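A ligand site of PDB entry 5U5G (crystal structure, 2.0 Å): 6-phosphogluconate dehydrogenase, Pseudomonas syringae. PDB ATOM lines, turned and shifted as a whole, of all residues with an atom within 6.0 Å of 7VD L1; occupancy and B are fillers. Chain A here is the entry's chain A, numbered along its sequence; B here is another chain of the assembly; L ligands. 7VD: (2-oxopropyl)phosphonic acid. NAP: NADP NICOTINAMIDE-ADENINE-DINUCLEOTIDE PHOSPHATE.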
ATOM      1  N   MET A  13       5.822  30.624 -17.562  1.00  0.00           N
ATOM      2  CA  MET A  13       6.134  30.796 -18.981  1.00  0.00           C
ATOM      3  C   MET A  13       6.174  32.262 -19.364  1.00  0.00           C
ATOM      4  O   MET A  13       7.041  32.687 -20.137  1.00  0.00           O
ATOM      5  CB  MET A  13       5.099  30.055 -19.841  1.00  0.00           C
ATOM      6  CG  MET A  13       5.308  30.194 -21.354  1.00  0.00           C
ATOM      7  SD  MET A  13       6.876  29.437 -21.874  1.00  0.00           S
ATOM      8  CE  MET A  13       6.642  27.829 -21.200  1.00  0.00           C
ATOM      9  N   THR A  98      -2.804  28.281 -23.546  1.00  0.00           N
ATOM     10  CA  THR A  98      -3.525  27.131 -24.041  1.00  0.00           C
ATOM     11  C   THR A  98      -4.957  27.222 -23.522  1.00  0.00           C
ATOM     12  O   THR A  98      -5.192  27.177 -22.313  1.00  0.00           O
ATOM     13  CB  THR A  98      -2.862  25.821 -23.615  1.00  0.00           C
ATOM     14  OG1 THR A  98      -1.497  25.838 -24.057  1.00  0.00           O
ATOM     15  CG2 THR A  98      -3.581  24.651 -24.266  1.00  0.00           C
ATOM     16  N   VAL A 123       2.191  27.640 -27.482  1.00  0.00           N
ATOM     17  CA  VAL A 123       3.614  27.351 -27.628  1.00  0.00           C
ATOM     18  C   VAL A 123       3.979  26.063 -26.910  1.00  0.00           C
ATOM     19  O   VAL A 123       3.225  25.557 -26.072  1.00  0.00           O
ATOM     20  CB  VAL A 123       4.485  28.511 -27.097  1.00  0.00           C
ATOM     21  CG1 VAL A 123       4.263  29.779 -27.915  1.00  0.00           C
ATOM     22  CG2 VAL A 123       4.202  28.747 -25.610  1.00  0.00           C
ATOM     23  N   SER A 124       5.148  25.527 -27.255  1.00  0.00           N
ATOM     24  CA  SER A 124       5.652  24.324 -26.597  1.00  0.00           C
ATOM     25  C   SER A 124       7.167  24.419 -26.495  1.00  0.00           C
ATOM     26  O   SER A 124       7.837  24.930 -27.392  1.00  0.00           O
ATOM     27  CB  SER A 124       5.233  23.060 -27.349  1.00  0.00           C
ATOM     28  OG  SER A 124       5.584  21.898 -26.641  1.00  0.00           O
ATOM     29  N   GLY A 125       7.698  23.901 -25.392  1.00  0.00           N
ATOM     30  CA  GLY A 125       9.136  23.948 -25.180  1.00  0.00           C
ATOM     31  C   GLY A 125       9.491  24.288 -23.753  1.00  0.00           C
ATOM     32  O   GLY A 125      10.670  24.237 -23.380  1.00  0.00           O
ATOM     33  N   GLY A 126       8.494  24.639 -22.944  1.00  0.00           N
ATOM     34  CA  GLY A 126       8.700  24.907 -21.529  1.00  0.00           C
ATOM     35  C   GLY A 126       9.506  26.175 -21.257  1.00  0.00           C
ATOM     36  O   GLY A 126       9.949  26.883 -22.158  1.00  0.00           O
ATOM     37  N   VAL A 127       9.659  26.462 -19.965  1.00  0.00           N
ATOM     38  CA  VAL A 127      10.475  27.593 -19.504  1.00  0.00           C
ATOM     39  C   VAL A 127      11.870  27.522 -20.119  1.00  0.00           C
ATOM     40  O   VAL A 127      12.413  28.534 -20.571  1.00  0.00           O
ATOM     41  CB  VAL A 127      10.524  27.612 -17.967  1.00  0.00           C
ATOM     42  CG1 VAL A 127      11.673  28.493 -17.456  1.00  0.00           C
ATOM     43  CG2 VAL A 127       9.192  28.075 -17.384  1.00  0.00           C
ATOM     44  N   LEU A 135      11.332  28.080 -28.573  1.00  0.00           N
ATOM     45  CA  LEU A 135       9.983  27.532 -28.471  1.00  0.00           C
ATOM     46  C   LEU A 135       9.454  27.144 -29.851  1.00  0.00           C
ATOM     47  O   LEU A 135       9.888  27.676 -30.876  1.00  0.00           O
ATOM     48  CB  LEU A 135       9.004  28.518 -27.832  1.00  0.00           C
ATOM     49  CG  LEU A 135       9.182  28.769 -26.327  1.00  0.00           C
ATOM     50  CD1 LEU A 135       8.221  29.845 -25.836  1.00  0.00           C
ATOM     51  CD2 LEU A 135       9.041  27.475 -25.530  1.00  0.00           C
ATOM     52  N   LYS A 173      -2.416  21.990 -30.261  1.00  0.00           N
ATOM     53  CA  LYS A 173      -1.675  22.094 -28.998  1.00  0.00           C
ATOM     54  C   LYS A 173      -2.226  21.117 -27.965  1.00  0.00           C
ATOM     55  O   LYS A 173      -1.447  20.426 -27.293  1.00  0.00           O
ATOM     56  CB  LYS A 173      -1.748  23.533 -28.475  1.00  0.00           C
ATOM     57  CG  LYS A 173      -1.298  23.713 -27.001  1.00  0.00           C
ATOM     58  CD  LYS A 173       0.234  23.548 -26.838  1.00  0.00           C
ATOM     59  CE  LYS A 173       0.667  23.734 -25.348  1.00  0.00           C
ATOM     60  NZ  LYS A 173       2.069  23.245 -25.105  1.00  0.00           N
ATOM     61  N   ASN A 176      -1.157  17.707 -28.834  1.00  0.00           N
ATOM     62  CA  ASN A 176       0.261  17.611 -28.511  1.00  0.00           C
ATOM     63  C   ASN A 176       0.468  17.321 -27.034  1.00  0.00           C
ATOM     64  O   ASN A 176       1.262  16.441 -26.664  1.00  0.00           O
ATOM     65  CB  ASN A 176       0.970  18.915 -28.895  1.00  0.00           C
ATOM     66  CG  ASN A 176       2.388  18.953 -28.406  1.00  0.00           C
ATOM     67  OD1 ASN A 176       3.287  18.422 -29.054  1.00  0.00           O
ATOM     68  ND2 ASN A 176       2.607  19.591 -27.248  1.00  0.00           N
ATOM     69  N   ASN A 177      -0.283  18.021 -26.170  1.00  0.00           N
ATOM     70  CA  ASN A 177      -0.073  17.925 -24.738  1.00  0.00           C
ATOM     71  C   ASN A 177      -0.663  16.649 -24.149  1.00  0.00           C
ATOM     72  O   ASN A 177      -0.167  16.167 -23.126  1.00  0.00           O
ATOM     73  CB  ASN A 177      -0.656  19.151 -24.039  1.00  0.00           C
ATOM     74  CG  ASN A 177       0.282  20.324 -24.099  1.00  0.00           C
ATOM     75  OD1 ASN A 177       1.006  20.493 -25.091  1.00  0.00           O
ATOM     76  ND2 ASN A 177       0.307  21.120 -23.037  1.00  0.00           N
ATOM     77  N   GLU A 180       2.203  14.447 -24.601  1.00  0.00           N
ATOM     78  CA  GLU A 180       3.125  14.745 -23.515  1.00  0.00           C
ATOM     79  C   GLU A 180       2.750  13.973 -22.258  1.00  0.00           C
ATOM     80  O   GLU A 180       3.599  13.341 -21.616  1.00  0.00           O
ATOM     81  CB  GLU A 180       3.108  16.247 -23.193  1.00  0.00           C
ATOM     82  CG  GLU A 180       3.549  17.143 -24.320  1.00  0.00           C
ATOM     83  CD  GLU A 180       3.591  18.611 -23.916  1.00  0.00           C
ATOM     84  OE1 GLU A 180       2.966  18.942 -22.888  1.00  0.00           O
ATOM     85  OE2 GLU A 180       4.246  19.411 -24.621  1.00  0.00           O
ATOM     86  N   TYR A 217       9.458  14.343 -23.275  1.00  0.00           N
ATOM     87  CA  TYR A 217       9.052  14.280 -21.871  1.00  0.00           C
ATOM     88  C   TYR A 217       9.742  13.180 -21.078  1.00  0.00           C
ATOM     89  O   TYR A 217       9.736  13.248 -19.839  1.00  0.00           O
ATOM     90  CB  TYR A 217       7.528  14.160 -21.749  1.00  0.00           C
ATOM     91  CG  TYR A 217       6.979  15.534 -21.449  1.00  0.00           C
ATOM     92  CD1 TYR A 217       6.844  16.485 -22.478  1.00  0.00           C
ATOM     93  CD2 TYR A 217       6.701  15.936 -20.146  1.00  0.00           C
ATOM     94  CE1 TYR A 217       6.395  17.778 -22.200  1.00  0.00           C
ATOM     95  CE2 TYR A 217       6.228  17.229 -19.869  1.00  0.00           C
ATOM     96  CZ  TYR A 217       6.089  18.144 -20.905  1.00  0.00           C
ATOM     97  OH  TYR A 217       5.636  19.434 -20.636  1.00  0.00           O
ATOM     98  N   VAL A 234       6.179  23.089 -14.854  1.00  0.00           N
ATOM     99  CA  VAL A 234       4.799  22.857 -15.225  1.00  0.00           C
ATOM    100  C   VAL A 234       4.079  22.334 -14.000  1.00  0.00           C
ATOM    101  O   VAL A 234       4.357  21.227 -13.514  1.00  0.00           O
ATOM    102  CB  VAL A 234       4.659  21.874 -16.394  1.00  0.00           C
ATOM    103  CG1 VAL A 234       3.184  21.793 -16.796  1.00  0.00           C
ATOM    104  CG2 VAL A 234       5.521  22.305 -17.573  1.00  0.00           C
ATOM    105  N   VAL A 238      -1.669  23.436 -14.388  1.00  0.00           N
ATOM    106  CA  VAL A 238      -1.574  23.683 -15.825  1.00  0.00           C
ATOM    107  C   VAL A 238      -1.742  22.393 -16.617  1.00  0.00           C
ATOM    108  O   VAL A 238      -2.453  22.343 -17.625  1.00  0.00           O
ATOM    109  CB  VAL A 238      -0.243  24.390 -16.157  1.00  0.00           C
ATOM    110  CG1 VAL A 238       0.108  24.235 -17.624  1.00  0.00           C
ATOM    111  CG2 VAL A 238      -0.335  25.879 -15.785  1.00  0.00           C
ATOM    112  N   ARG A 239      -1.084  21.323 -16.158  1.00  0.00           N
ATOM    113  CA  ARG A 239      -1.187  20.029 -16.837  1.00  0.00           C
ATOM    114  C   ARG A 239      -2.626  19.546 -16.874  1.00  0.00           C
ATOM    115  O   ARG A 239      -3.126  19.125 -17.928  1.00  0.00           O
ATOM    116  CB  ARG A 239      -0.278  19.012 -16.136  1.00  0.00           C
ATOM    117  CG  ARG A 239      -0.220  17.636 -16.816  1.00  0.00           C
ATOM    118  CD  ARG A 239       1.068  17.509 -17.631  1.00  0.00           C
ATOM    119  NE  ARG A 239       0.778  17.675 -19.033  1.00  0.00           N
ATOM    120  CZ  ARG A 239       1.622  18.138 -19.951  1.00  0.00           C
ATOM    121  NH1 ARG A 239       2.850  18.535 -19.639  1.00  0.00           N
ATOM    122  NH2 ARG A 239       1.213  18.222 -21.212  1.00  0.00           N
ATOM    123  N   ASP A 242      -5.018  21.315 -19.280  1.00  0.00           N
ATOM    124  CA  ASP A 242      -4.924  20.868 -20.659  1.00  0.00           C
ATOM    125  C   ASP A 242      -5.556  19.485 -20.844  1.00  0.00           C
ATOM    126  O   ASP A 242      -6.220  19.233 -21.850  1.00  0.00           O
ATOM    127  CB  ASP A 242      -3.463  20.879 -21.127  1.00  0.00           C
ATOM    128  CG  ASP A 242      -2.891  22.295 -21.197  1.00  0.00           C
ATOM    129  OD1 ASP A 242      -3.689  23.268 -21.094  1.00  0.00           O
ATOM    130  OD2 ASP A 242      -1.657  22.444 -21.345  1.00  0.00           O
ATOM    131  N   GLN A 279       4.221  18.607 -12.188  1.00  0.00           N
ATOM    132  CA  GLN A 279       3.650  17.512 -12.978  1.00  0.00           C
ATOM    133  C   GLN A 279       4.380  16.189 -12.716  1.00  0.00           C
ATOM    134  O   GLN A 279       3.757  15.125 -12.730  1.00  0.00           O
ATOM    135  CB  GLN A 279       3.700  17.862 -14.472  1.00  0.00           C
ATOM    136  CG  GLN A 279       5.100  18.242 -14.969  1.00  0.00           C
ATOM    137  CD  GLN A 279       5.180  18.530 -16.451  1.00  0.00           C
ATOM    138  OE1 GLN A 279       4.189  18.383 -17.185  1.00  0.00           O
ATOM    139  NE2 GLN A 279       6.356  18.961 -16.907  1.00  0.00           N
ATOM    140  N   CYS B 211       6.888  20.298 -31.358  1.00  0.00           N
ATOM    141  CA  CYS B 211       6.467  20.515 -29.978  1.00  0.00           C
ATOM    142  C   CYS B 211       6.813  19.302 -29.119  1.00  0.00           C
ATOM    143  O   CYS B 211       7.185  18.234 -29.606  1.00  0.00           O
ATOM    144  CB  CYS B 211       4.970  20.804 -29.939  1.00  0.00           C
ATOM    145  SG  CYS B 211       4.478  22.276 -30.896  1.00  0.00           S
ATOM    146  N   ARG B 212       6.684  19.474 -27.801  1.00  0.00           N
ATOM    147  CA  ARG B 212       7.211  18.488 -26.844  1.00  0.00           C
ATOM    148  C   ARG B 212       6.329  17.254 -26.657  1.00  0.00           C
ATOM    149  O   ARG B 212       6.606  16.456 -25.750  1.00  0.00           O
ATOM    150  CB  ARG B 212       7.422  19.140 -25.480  1.00  0.00           C
ATOM    151  CG  ARG B 212       8.628  20.030 -25.390  1.00  0.00           C
ATOM    152  CD  ARG B 212       8.484  20.767 -24.070  1.00  0.00           C
ATOM    153  NE  ARG B 212       9.640  20.590 -23.266  1.00  0.00           N
ATOM    154  CZ  ARG B 212       9.744  20.876 -21.976  1.00  0.00           C
ATOM    155  NH1 ARG B 212       8.733  21.379 -21.268  1.00  0.00           N
ATOM    156  NH2 ARG B 212      10.897  20.628 -21.409  1.00  0.00           N
ATOM    157  N   GLY B 213       5.298  17.061 -27.470  1.00  0.00           N
ATOM    158  CA  GLY B 213       4.767  15.715 -27.539  1.00  0.00           C
ATOM    159  C   GLY B 213       5.572  14.784 -28.451  1.00  0.00           C
ATOM    160  O   GLY B 213       5.194  13.622 -28.624  1.00  0.00           O
HETATM  161  P1  7VD L   1       5.246  22.213 -22.959  1.00  0.00           P
HETATM  162  C1  7VD L   1       4.359  22.496 -21.406  1.00  0.00           C
HETATM  163  O2  7VD L   1       4.361  21.882 -24.128  1.00  0.00           O
HETATM  164  O3  7VD L   1       6.147  23.367 -23.308  1.00  0.00           O
HETATM  165  O4  7VD L   1       6.068  21.015 -22.566  1.00  0.00           O
HETATM  166  C6  7VD L   1       2.857  22.623 -21.496  1.00  0.00           C
HETATM  167  O7  7VD L   1       2.325  23.168 -22.460  1.00  0.00           O
HETATM  168  C8  7VD L   1       2.080  22.034 -20.349  1.00  0.00           C
HETATM  169  PA  NAP L   2       1.328  29.871 -14.025  1.00  0.00           P
HETATM  170  O1A NAP L   2       0.362  29.166 -13.133  1.00  0.00           O
HETATM  171  O2A NAP L   2       2.809  29.815 -13.757  1.00  0.00           O
HETATM  172  O5B NAP L   2       0.888  31.461 -14.183  1.00  0.00           O
HETATM  173  C5B NAP L   2      -0.476  31.491 -14.514  1.00  0.00           C
HETATM  174  C4B NAP L   2      -0.784  32.937 -14.972  1.00  0.00           C
HETATM  175  O4B NAP L   2      -2.187  33.116 -15.195  1.00  0.00           O
HETATM  176  C3B NAP L   2      -0.293  33.954 -13.885  1.00  0.00           C
HETATM  177  O3B NAP L   2       0.125  35.120 -14.507  1.00  0.00           O
HETATM  178  C2B NAP L   2      -1.621  34.237 -13.151  1.00  0.00           C
HETATM  179  O2B NAP L   2      -1.709  35.454 -12.580  1.00  0.00           O
HETATM  180  C1B NAP L   2      -2.572  34.227 -14.408  1.00  0.00           C
HETATM  181  N9A NAP L   2      -3.945  34.054 -13.948  1.00  0.00           N
HETATM  182  C8A NAP L   2      -4.618  32.877 -13.571  1.00  0.00           C
HETATM  183  N7A NAP L   2      -5.896  33.107 -13.162  1.00  0.00           N
HETATM  184  C5A NAP L   2      -6.029  34.492 -13.265  1.00  0.00           C
HETATM  185  C6A NAP L   2      -7.102  35.361 -12.990  1.00  0.00           C
HETATM  186  N6A NAP L   2      -8.303  34.876 -12.525  1.00  0.00           N
HETATM  187  N1A NAP L   2      -6.990  36.710 -13.171  1.00  0.00           N
HETATM  188  C2A NAP L   2      -5.780  37.144 -13.631  1.00  0.00           C
HETATM  189  N3A NAP L   2      -4.675  36.448 -13.954  1.00  0.00           N
HETATM  190  C4A NAP L   2      -4.825  35.097 -13.756  1.00  0.00           C
HETATM  191  O3  NAP L   2       0.949  29.088 -15.428  1.00  0.00           O
HETATM  192  PN  NAP L   2       2.152  28.985 -16.482  1.00  0.00           P
HETATM  193  O1N NAP L   2       2.819  30.273 -16.738  1.00  0.00           O
HETATM  194  O2N NAP L   2       2.875  27.662 -16.425  1.00  0.00           O
HETATM  195  O5D NAP L   2       1.262  28.725 -17.955  1.00  0.00           O
HETATM  196  C5D NAP L   2       0.735  29.883 -18.447  1.00  0.00           C
HETATM  197  C4D NAP L   2       0.173  29.549 -19.811  1.00  0.00           C
HETATM  198  O4D NAP L   2       1.223  29.034 -20.670  1.00  0.00           O
HETATM  199  C3D NAP L   2      -0.900  28.396 -19.679  1.00  0.00           C
HETATM  200  O3D NAP L   2      -1.937  28.638 -20.595  1.00  0.00           O
HETATM  201  C2D NAP L   2      -0.125  27.157 -20.049  1.00  0.00           C
HETATM  202  O2D NAP L   2      -0.914  26.158 -20.633  1.00  0.00           O
HETATM  203  C1D NAP L   2       0.830  27.750 -21.135  1.00  0.00           C
HETATM  204  N1N NAP L   2       2.023  26.951 -21.281  1.00  0.00           N
HETATM  205  C2N NAP L   2       2.878  26.672 -20.180  1.00  0.00           C
HETATM  206  C3N NAP L   2       4.052  25.973 -20.403  1.00  0.00           C
HETATM  207  C7N NAP L   2       4.968  25.688 -19.303  1.00  0.00           C
HETATM  208  O7N NAP L   2       6.041  25.111 -19.462  1.00  0.00           O
HETATM  209  N7N NAP L   2       4.666  26.132 -18.018  1.00  0.00           N
HETATM  210  C4N NAP L   2       4.460  25.526 -21.779  1.00  0.00           C
HETATM  211  C5N NAP L   2       3.492  25.863 -22.832  1.00  0.00           C
HETATM  212  C6N NAP L   2       2.358  26.511 -22.570  1.00  0.00           C
HETATM  213  P2B NAP L   2      -1.006  35.563 -10.873  1.00  0.00           P
HETATM  214  O1X NAP L   2       0.454  35.552 -11.228  1.00  0.00           O
HETATM  215  O2X NAP L   2      -1.588  36.886 -10.364  1.00  0.00           O
HETATM  216  O3X NAP L   2      -1.581  34.294 -10.293  1.00  0.00           O
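The side-chain hydroxyl (OG) of Ser 124 lies within hydrogen-bond range of an oxygen (O2) of 7VD L1 (2.8 Å). An oxygen (O7) of 7VD L1 sits at hydrogen-bond distance from the side-chain amide nitrogen (ND2) of Asn 177 (2.9 Å). The side-chain amino group (NZ) of Lys 173 lies within salt-bridge range of an oxygen (O2) of 7VD L1. N of Thr 98 lies within hydrogen-bond range of O3D of NAP L2 (3.1 Å). An oxygen (O3) of 7VD L1 is in hydrogen-bond range of the backbone NH (N) of Gly 125. O4 of 7VD L1 is in salt-bridge range of NH1 of Arg 212 of chain B, 3.0 Å away. The side-chain hydroxyl (OG1) of Thr 98 is in hydrogen-bond range of an oxygen (O2D) of NAP L2 (3.5 Å). The side-chain carboxylate (OE2) of Glu 180 sits close to an oxygen (O2) of 7VD L1 (2.5 Å). An oxygen (O4) of 7VD L1 sits at hydrogen-bond distance from the side-chain hydroxyl of Tyr 217 (2.5 Å). The backbone NH of Met 13 lies within hydrogen-bond range of an oxygen (O1N) of NAP L2 (3.1 Å). The backbone NH (N) of Gly 126 lies within hydrogen-bond range of an oxygen (O3) of 7VD L1, 2.7 Å away.
Val 234 touches 7VD L1. NH1 of Arg 239 touches C8 of 7VD L1, at 3.7 Å. OD2 of Asp 242 touches C8 of 7VD L1 (3.9 Å). Hydrophobic or aromatic side chains within 4 Å of 7VD L1: Tyr 217 and Val 234. Of the 21 residues printed, 11 come within 4 Å of 7VD L1. Along chain A the residues within 4 Å of 7VD L1 span positions 124 to 242. The nearest printed residue that does not touch 7VD L1 is Val 238 (4.02 Å).
The side-chain hydroxyl (OG) of Ser 124 is in hydrogen-bond range of the backbone NH (N) of Arg 212 of chain B (2.9 Å). The side-chain amide oxygen (OD1) of Asn 177 is in hydrogen-bond range of the side-chain amide nitrogen (ND2) of Asn 176 (2.8 Å). The backbone carbonyl oxygen (O) of Val 234 sits at hydrogen-bond distance from the backbone NH (N) of Gln 279 (2.9 Å). The side-chain carboxylate (OE2) of Glu 180 sits at hydrogen-bond distance from the side-chain amide nitrogen (ND2) of Asn 176 (3.1 Å). OD2 of Asp 242 sits at hydrogen-bond distance from ND2 of Asn 177. The backbone carbonyl oxygen (O) of Asn 177 sits at hydrogen-bond distance from the guanidinium group (NH2) of Arg 239 (3.1 Å). NH1 of Arg 239 is in hydrogen-bond range of OE1 of Gln 279, at 2.8 Å. The side-chain carboxylate (OE2) of Glu 180 lies within hydrogen-bond range of the side-chain hydroxyl (OG) of Ser 124.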
